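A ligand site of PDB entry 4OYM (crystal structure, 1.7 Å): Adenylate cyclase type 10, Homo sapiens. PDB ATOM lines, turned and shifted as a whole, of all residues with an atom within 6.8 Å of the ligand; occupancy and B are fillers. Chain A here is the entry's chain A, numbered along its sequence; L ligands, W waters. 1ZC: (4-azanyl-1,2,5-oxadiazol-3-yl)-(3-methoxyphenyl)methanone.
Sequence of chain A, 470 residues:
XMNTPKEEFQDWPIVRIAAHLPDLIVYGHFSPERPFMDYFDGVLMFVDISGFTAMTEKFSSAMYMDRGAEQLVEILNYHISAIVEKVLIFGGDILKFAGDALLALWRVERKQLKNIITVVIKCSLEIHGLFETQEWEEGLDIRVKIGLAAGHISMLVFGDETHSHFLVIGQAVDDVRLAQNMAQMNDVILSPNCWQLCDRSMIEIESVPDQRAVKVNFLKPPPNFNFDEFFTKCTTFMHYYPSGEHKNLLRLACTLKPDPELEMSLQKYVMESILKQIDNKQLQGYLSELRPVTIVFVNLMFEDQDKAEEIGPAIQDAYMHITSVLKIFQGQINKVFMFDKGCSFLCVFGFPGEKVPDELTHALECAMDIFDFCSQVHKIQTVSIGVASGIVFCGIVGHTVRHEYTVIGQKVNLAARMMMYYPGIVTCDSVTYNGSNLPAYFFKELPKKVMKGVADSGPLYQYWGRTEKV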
ATOM      1  N   PHE A  46       2.569 -16.165  28.253  1.00  0.00           N
ATOM      2  CA  PHE A  46       2.028 -17.022  29.328  1.00  0.00           C
ATOM      3  C   PHE A  46       2.844 -16.786  30.550  1.00  0.00           C
ATOM      4  O   PHE A  46       4.039 -17.068  30.538  1.00  0.00           O
ATOM      5  CB  PHE A  46       2.071 -18.486  28.898  1.00  0.00           C
ATOM      6  CG  PHE A  46       1.157 -19.415  29.660  1.00  0.00           C
ATOM      7  CD1 PHE A  46      -0.212 -19.180  29.710  1.00  0.00           C
ATOM      8  CD2 PHE A  46       1.655 -20.560  30.264  1.00  0.00           C
ATOM      9  CE1 PHE A  46      -1.063 -20.049  30.391  1.00  0.00           C
ATOM     10  CE2 PHE A  46       0.809 -21.429  30.954  1.00  0.00           C
ATOM     11  CZ  PHE A  46      -0.553 -21.173  31.001  1.00  0.00           C
ATOM     12  N   VAL A  47       2.224 -16.244  31.614  1.00  0.00           N
ATOM     13  CA  VAL A  47       2.940 -15.850  32.848  1.00  0.00           C
ATOM     14  C   VAL A  47       2.515 -16.870  33.874  1.00  0.00           C
ATOM     15  O   VAL A  47       1.327 -16.912  34.231  1.00  0.00           O
ATOM     16  CB  VAL A  47       2.626 -14.398  33.340  1.00  0.00           C
ATOM     17  CG1 VAL A  47       3.503 -13.999  34.541  1.00  0.00           C
ATOM     18  CG2 VAL A  47       2.765 -13.380  32.214  1.00  0.00           C
ATOM     19  N   LEU A  95      -6.208 -12.414  28.016  1.00  0.00           N
ATOM     20  CA  LEU A  95      -7.263 -13.355  27.569  1.00  0.00           C
ATOM     21  C   LEU A  95      -7.962 -14.062  28.686  1.00  0.00           C
ATOM     22  O   LEU A  95      -9.198 -14.082  28.693  1.00  0.00           O
ATOM     23  CB  LEU A  95      -6.676 -14.418  26.601  1.00  0.00           C
ATOM     24  CG  LEU A  95      -6.148 -13.872  25.263  1.00  0.00           C
ATOM     25  CD1 LEU A  95      -5.764 -15.024  24.315  1.00  0.00           C
ATOM     26  CD2 LEU A  95      -7.182 -12.875  24.609  1.00  0.00           C
ATOM     27  N   LYS A  96      -7.206 -14.637  29.628  1.00  0.00           N
ATOM     28  CA  LYS A  96      -7.788 -15.484  30.685  1.00  0.00           C
ATOM     29  C   LYS A  96      -6.835 -15.561  31.869  1.00  0.00           C
ATOM     30  O   LYS A  96      -5.607 -15.452  31.674  1.00  0.00           O
ATOM     31  CB  LYS A  96      -7.967 -16.929  30.135  1.00  0.00           C
ATOM     32  CG  LYS A  96      -9.244 -17.130  29.348  1.00  0.00           C
ATOM     33  CD  LYS A  96      -9.771 -18.552  29.408  1.00  0.00           C
ATOM     34  CE  LYS A  96     -10.440 -18.821  28.087  1.00  0.00           C
ATOM     35  NZ  LYS A  96     -11.488 -19.844  28.204  1.00  0.00           N
ATOM     36  N   PHE A  97      -7.405 -15.758  33.065  1.00  0.00           N
ATOM     37  CA  PHE A  97      -6.687 -16.031  34.309  1.00  0.00           C
ATOM     38  C   PHE A  97      -7.038 -17.464  34.724  1.00  0.00           C
ATOM     39  O   PHE A  97      -8.173 -17.923  34.561  1.00  0.00           O
ATOM     40  CB  PHE A  97      -7.151 -15.087  35.450  1.00  0.00           C
ATOM     41  CG  PHE A  97      -6.898 -13.621  35.235  1.00  0.00           C
ATOM     42  CD1 PHE A  97      -7.839 -12.824  34.584  1.00  0.00           C
ATOM     43  CD2 PHE A  97      -5.734 -13.019  35.738  1.00  0.00           C
ATOM     44  CE1 PHE A  97      -7.604 -11.438  34.401  1.00  0.00           C
ATOM     45  CE2 PHE A  97      -5.500 -11.647  35.554  1.00  0.00           C
ATOM     46  CZ  PHE A  97      -6.441 -10.870  34.889  1.00  0.00           C
ATOM     47  N   ALA A  98      -6.035 -18.171  35.273  1.00  0.00           N
ATOM     48  CA  ALA A  98      -6.292 -19.405  36.021  1.00  0.00           C
ATOM     49  C   ALA A  98      -5.529 -19.293  37.323  1.00  0.00           C
ATOM     50  O   ALA A  98      -4.742 -18.357  37.481  1.00  0.00           O
ATOM     51  CB  ALA A  98      -5.778 -20.591  35.237  1.00  0.00           C
ATOM     52  N   GLY A  99      -5.771 -20.239  38.219  1.00  0.00           N
ATOM     53  CA  GLY A  99      -4.987 -20.412  39.433  1.00  0.00           C
ATOM     54  C   GLY A  99      -3.498 -20.260  39.247  1.00  0.00           C
ATOM     55  O   GLY A  99      -2.873 -19.555  40.035  1.00  0.00           O
ATOM     56  N   ASP A 100      -2.914 -20.873  38.204  1.00  0.00           N
ATOM     57  CA  ASP A 100      -1.462 -20.929  38.093  1.00  0.00           C
ATOM     58  C   ASP A 100      -0.900 -20.047  36.940  1.00  0.00           C
ATOM     59  O   ASP A 100       0.313 -19.949  36.831  1.00  0.00           O
ATOM     60  CB  ASP A 100      -0.977 -22.374  38.009  1.00  0.00           C
ATOM     61  CG  ASP A 100      -1.453 -23.252  39.172  1.00  0.00           C
ATOM     62  OD1 ASP A 100      -2.682 -23.402  39.340  1.00  0.00           O
ATOM     63  OD2 ASP A 100      -0.585 -23.775  39.911  1.00  0.00           O
ATOM     64  N   ALA A 101      -1.749 -19.391  36.111  1.00  0.00           N
ATOM     65  CA  ALA A 101      -1.269 -18.615  34.975  1.00  0.00           C
ATOM     66  C   ALA A 101      -2.156 -17.483  34.510  1.00  0.00           C
ATOM     67  O   ALA A 101      -3.361 -17.443  34.810  1.00  0.00           O
ATOM     68  CB  ALA A 101      -1.018 -19.538  33.807  1.00  0.00           C
ATOM     69  N   LEU A 102      -1.565 -16.539  33.753  1.00  0.00           N
ATOM     70  CA  LEU A 102      -2.445 -15.719  32.921  1.00  0.00           C
ATOM     71  C   LEU A 102      -1.910 -15.742  31.496  1.00  0.00           C
ATOM     72  O   LEU A 102      -0.717 -15.901  31.295  1.00  0.00           O
ATOM     73  CB  LEU A 102      -2.637 -14.294  33.471  1.00  0.00           C
ATOM     74  CG  LEU A 102      -1.440 -13.373  33.599  1.00  0.00           C
ATOM     75  CD1 LEU A 102      -1.106 -12.673  32.253  1.00  0.00           C
ATOM     76  CD2 LEU A 102      -1.765 -12.242  34.625  1.00  0.00           C
ATOM     77  N   LEU A 103      -2.785 -15.587  30.524  1.00  0.00           N
ATOM     78  CA  LEU A 103      -2.393 -15.616  29.130  1.00  0.00           C
ATOM     79  C   LEU A 103      -2.760 -14.289  28.517  1.00  0.00           C
ATOM     80  O   LEU A 103      -3.913 -13.832  28.685  1.00  0.00           O
ATOM     81  CB  LEU A 103      -3.182 -16.754  28.432  1.00  0.00           C
ATOM     82  CG  LEU A 103      -2.997 -16.890  26.911  1.00  0.00           C
ATOM     83  CD1 LEU A 103      -1.530 -17.295  26.562  1.00  0.00           C
ATOM     84  CD2 LEU A 103      -3.954 -17.946  26.320  1.00  0.00           C
ATOM     85  N   ALA A 104      -1.799 -13.656  27.823  1.00  0.00           N
ATOM     86  CA  ALA A 104      -2.047 -12.371  27.155  1.00  0.00           C
ATOM     87  C   ALA A 104      -1.705 -12.492  25.667  1.00  0.00           C
ATOM     88  O   ALA A 104      -0.832 -13.291  25.269  1.00  0.00           O
ATOM     89  CB  ALA A 104      -1.214 -11.237  27.782  1.00  0.00           C
ATOM     90  N   PHE A 166     -14.981 -18.958  25.201  1.00  0.00           N
ATOM     91  CA  PHE A 166     -14.025 -18.896  24.106  1.00  0.00           C
ATOM     92  C   PHE A 166     -12.714 -19.586  24.476  1.00  0.00           C
ATOM     93  O   PHE A 166     -12.399 -19.754  25.666  1.00  0.00           O
ATOM     94  CB  PHE A 166     -13.772 -17.445  23.652  1.00  0.00           C
ATOM     95  CG  PHE A 166     -12.775 -16.734  24.550  1.00  0.00           C
ATOM     96  CD1 PHE A 166     -11.419 -16.712  24.228  1.00  0.00           C
ATOM     97  CD2 PHE A 166     -13.177 -16.119  25.720  1.00  0.00           C
ATOM     98  CE1 PHE A 166     -10.489 -16.067  25.058  1.00  0.00           C
ATOM     99  CE2 PHE A 166     -12.257 -15.459  26.559  1.00  0.00           C
ATOM    100  CZ  PHE A 166     -10.920 -15.458  26.224  1.00  0.00           C
ATOM    101  N   LEU A 167     -11.950 -19.936  23.468  1.00  0.00           N
ATOM    102  CA  LEU A 167     -10.609 -20.511  23.550  1.00  0.00           C
ATOM    103  C   LEU A 167      -9.776 -19.997  22.407  1.00  0.00           C
ATOM    104  O   LEU A 167     -10.301 -19.766  21.304  1.00  0.00           O
ATOM    105  CB  LEU A 167     -10.705 -22.036  23.370  1.00  0.00           C
ATOM    106  CG  LEU A 167     -11.163 -22.856  24.511  1.00  0.00           C
ATOM    107  CD1 LEU A 167     -11.351 -24.305  24.043  1.00  0.00           C
ATOM    108  CD2 LEU A 167     -10.151 -22.797  25.648  1.00  0.00           C
ATOM    109  N   VAL A 168      -8.466 -19.788  22.658  1.00  0.00           N
ATOM    110  CA  VAL A 168      -7.526 -19.684  21.566  1.00  0.00           C
ATOM    111  C   VAL A 168      -6.814 -21.040  21.446  1.00  0.00           C
ATOM    112  O   VAL A 168      -6.474 -21.687  22.456  1.00  0.00           O
ATOM    113  CB  VAL A 168      -6.522 -18.514  21.631  1.00  0.00           C
ATOM    114  CG1 VAL A 168      -7.227 -17.186  21.369  1.00  0.00           C
ATOM    115  CG2 VAL A 168      -5.721 -18.516  22.933  1.00  0.00           C
ATOM    116  N   ILE A 169      -6.618 -21.469  20.206  1.00  0.00           N
ATOM    117  CA  ILE A 169      -6.007 -22.763  19.915  1.00  0.00           C
ATOM    118  C   ILE A 169      -4.965 -22.681  18.783  1.00  0.00           C
ATOM    119  O   ILE A 169      -4.849 -21.653  18.112  1.00  0.00           O
ATOM    120  CB  ILE A 169      -7.084 -23.864  19.660  1.00  0.00           C
ATOM    121  CG1 ILE A 169      -7.749 -23.648  18.285  1.00  0.00           C
ATOM    122  CG2 ILE A 169      -8.172 -23.952  20.789  1.00  0.00           C
ATOM    123  CD1 ILE A 169      -8.375 -24.897  17.708  1.00  0.00           C
ATOM    124  N   VAL A 173      -0.364 -21.342  20.453  1.00  0.00           N
ATOM    125  CA  VAL A 173      -0.968 -21.650  21.755  1.00  0.00           C
ATOM    126  C   VAL A 173      -0.239 -22.862  22.432  1.00  0.00           C
ATOM    127  O   VAL A 173       0.179 -22.754  23.590  1.00  0.00           O
ATOM    128  CB  VAL A 173      -2.513 -21.854  21.628  1.00  0.00           C
ATOM    129  CG1 VAL A 173      -3.120 -22.334  22.944  1.00  0.00           C
ATOM    130  CG2 VAL A 173      -3.188 -20.551  21.180  1.00  0.00           C
ATOM    131  N   ARG A 177       2.687 -22.629  26.041  1.00  0.00           N
ATOM    132  CA  ARG A 177       2.662 -23.496  27.206  1.00  0.00           C
ATOM    133  C   ARG A 177       3.982 -24.256  27.303  1.00  0.00           C
ATOM    134  O   ARG A 177       4.575 -24.276  28.384  1.00  0.00           O
ATOM    135  CB  ARG A 177       1.504 -24.519  27.105  1.00  0.00           C
ATOM    136  CG  ARG A 177       1.658 -25.705  28.075  1.00  0.00           C
ATOM    137  CD  ARG A 177       0.442 -26.000  28.909  1.00  0.00           C
ATOM    138  NE  ARG A 177       0.300 -25.106  30.056  1.00  0.00           N
ATOM    139  CZ  ARG A 177      -0.690 -25.177  30.951  1.00  0.00           C
ATOM    140  NH1 ARG A 177      -1.633 -26.096  30.822  1.00  0.00           N
ATOM    141  NH2 ARG A 177      -0.744 -24.327  31.967  1.00  0.00           N
ATOM    142  N   VAL A 336     -12.418 -22.931  30.762  1.00  0.00           N
ATOM    143  CA  VAL A 336     -12.091 -23.883  29.685  1.00  0.00           C
ATOM    144  C   VAL A 336     -10.713 -23.455  29.190  1.00  0.00           C
ATOM    145  O   VAL A 336     -10.476 -22.254  29.029  1.00  0.00           O
ATOM    146  CB  VAL A 336     -13.149 -23.926  28.533  1.00  0.00           C
ATOM    147  CG1 VAL A 336     -12.852 -25.045  27.541  1.00  0.00           C
ATOM    148  CG2 VAL A 336     -14.582 -24.028  29.056  1.00  0.00           C
ATOM    149  N   PHE A 337      -9.833 -24.419  28.962  1.00  0.00           N
ATOM    150  CA  PHE A 337      -8.415 -24.216  28.658  1.00  0.00           C
ATOM    151  C   PHE A 337      -8.053 -25.220  27.613  1.00  0.00           C
ATOM    152  O   PHE A 337      -8.632 -26.311  27.613  1.00  0.00           O
ATOM    153  CB  PHE A 337      -7.532 -24.583  29.871  1.00  0.00           C
ATOM    154  CG  PHE A 337      -7.737 -23.823  31.144  1.00  0.00           C
ATOM    155  CD1 PHE A 337      -7.768 -24.487  32.366  1.00  0.00           C
ATOM    156  CD2 PHE A 337      -7.857 -22.431  31.137  1.00  0.00           C
ATOM    157  CE1 PHE A 337      -7.919 -23.787  33.555  1.00  0.00           C
ATOM    158  CE2 PHE A 337      -8.007 -21.724  32.340  1.00  0.00           C
ATOM    159  CZ  PHE A 337      -8.027 -22.409  33.540  1.00  0.00           C
ATOM    160  N   MET A 338      -7.080 -24.896  26.750  1.00  0.00           N
ATOM    161  CA  MET A 338      -6.624 -25.855  25.751  1.00  0.00           C
ATOM    162  C   MET A 338      -5.203 -25.636  25.296  1.00  0.00           C
ATOM    163  O   MET A 338      -4.892 -24.579  24.770  1.00  0.00           O
ATOM    164  CB  MET A 338      -7.590 -25.868  24.534  1.00  0.00           C
ATOM    165  CG  MET A 338      -7.094 -26.753  23.448  1.00  0.00           C
ATOM    166  SD  MET A 338      -8.457 -27.159  22.458  1.00  0.00           S
ATOM    167  CE  MET A 338      -7.642 -28.196  21.311  1.00  0.00           C
ATOM    168  N   PHE A 339      -4.331 -26.646  25.495  1.00  0.00           N
ATOM    169  CA  PHE A 339      -2.929 -26.508  25.098  1.00  0.00           C
ATOM    170  C   PHE A 339      -2.391 -27.704  24.357  1.00  0.00           C
ATOM    171  O   PHE A 339      -2.221 -27.568  23.166  1.00  0.00           O
ATOM    172  CB  PHE A 339      -2.008 -26.158  26.274  1.00  0.00           C
ATOM    173  CG  PHE A 339      -2.114 -24.738  26.760  1.00  0.00           C
ATOM    174  CD1 PHE A 339      -2.555 -24.454  28.035  1.00  0.00           C
ATOM    175  CD2 PHE A 339      -1.758 -23.679  25.938  1.00  0.00           C
ATOM    176  CE1 PHE A 339      -2.636 -23.140  28.494  1.00  0.00           C
ATOM    177  CE2 PHE A 339      -1.839 -22.357  26.385  1.00  0.00           C
ATOM    178  CZ  PHE A 339      -2.286 -22.094  27.663  1.00  0.00           C
ATOM    179  N   SER A 344      -9.795 -28.728  28.109  1.00  0.00           N
ATOM    180  CA  SER A 344     -10.203 -29.115  29.458  1.00  0.00           C
ATOM    181  C   SER A 344     -11.230 -28.169  30.057  1.00  0.00           C
ATOM    182  O   SER A 344     -11.112 -26.947  29.962  1.00  0.00           O
ATOM    183  CB  SER A 344      -8.983 -29.281  30.361  1.00  0.00           C
ATOM    184  OG  SER A 344      -8.369 -28.038  30.672  1.00  0.00           O
HETATM  185  C1  1ZC L   1      -3.880 -23.206  32.626  1.00  0.00           C
HETATM  186  C3  1ZC L   1      -4.294 -21.038  31.686  1.00  0.00           C
HETATM  187  C5  1ZC L   1      -4.834 -18.822  30.957  1.00  0.00           C
HETATM  188  C6  1ZC L   1      -5.309 -19.323  29.761  1.00  0.00           C
HETATM  189  C7  1ZC L   1      -5.271 -20.691  29.504  1.00  0.00           C
HETATM  190  C8  1ZC L   1      -4.757 -21.539  30.482  1.00  0.00           C
HETATM  191  C11 1ZC L   1      -6.584 -20.580  27.255  1.00  0.00           C
HETATM  192  C15 1ZC L   1      -6.777 -21.008  25.918  1.00  0.00           C
HETATM  193  O2  1ZC L   1      -3.765 -21.790  32.710  1.00  0.00           O
HETATM  194  C4  1ZC L   1      -4.326 -19.670  31.926  1.00  0.00           C
HETATM  195  C9  1ZC L   1      -5.778 -21.308  28.249  1.00  0.00           C
HETATM  196  O10 1ZC L   1      -5.539 -22.491  28.019  1.00  0.00           O
HETATM  197  N12 1ZC L   1      -7.276 -19.483  27.442  1.00  0.00           N
HETATM  198  O13 1ZC L   1      -7.879 -19.235  26.223  1.00  0.00           O
HETATM  199  N14 1ZC L   1      -7.571 -20.174  25.298  1.00  0.00           N
HETATM  200  N16 1ZC L   1      -6.232 -22.093  25.343  1.00  0.00           N
HETATM  201  O   HOH W   1      -3.190 -22.444  35.718  1.00  0.00           O
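Merely in contact with the ligand: Phe 339, Lys 96, Phe 337, Arg 177, Ala 98, Leu 167, Leu 103, Phe 46, Ala 101 and Val 173.
Hydrophobic or aromatic side chains within 4 Å of the ligand: Phe 46, Ala 98, Ala 101, Leu 103, Leu 167, Val 168, Val 173, Phe 337 and Phe 339.
Of the 23 residues printed, 12 come within 4 Å of the ligand.
The nearest printed residue that does not touch the ligand is Phe 166 (4.3 Å).
Water W1 lies within hydrogen-bond range of N of Asp 100 (3.0 Å), O2 of the ligand (3.1 Å) and N of Ala 101 (3.4 Å).
O of Met 338 sits at hydrogen-bond distance from N16 of the ligand (2.9 Å).
A nitrogen (N14) of the ligand is in hydrogen-bond range of the backbone NH (N) of Val 168 (2.8 Å).
O of Val 168 lies within hydrogen-bond range of N16 of the ligand, 2.9 Å away.
The backbone NH of Met 338 sits at hydrogen-bond distance from an oxygen (O10) of the ligand (3.1 Å).
O of Val 336 is in hydrogen-bond range of NZ of Lys 96 (2.7 Å).
O of Lys 96 sits at hydrogen-bond distance from N of Leu 103 (3.1 Å).
The backbone carbonyl oxygen of Leu 103 is in hydrogen-bond range of the backbone NH of Leu 95 (2.8 Å).
NZ of Lys 96 sits at hydrogen-bond distance from O of Phe 166, at 2.7 Å.
N of Ser 344 lies within hydrogen-bond range of O of Phe 337.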
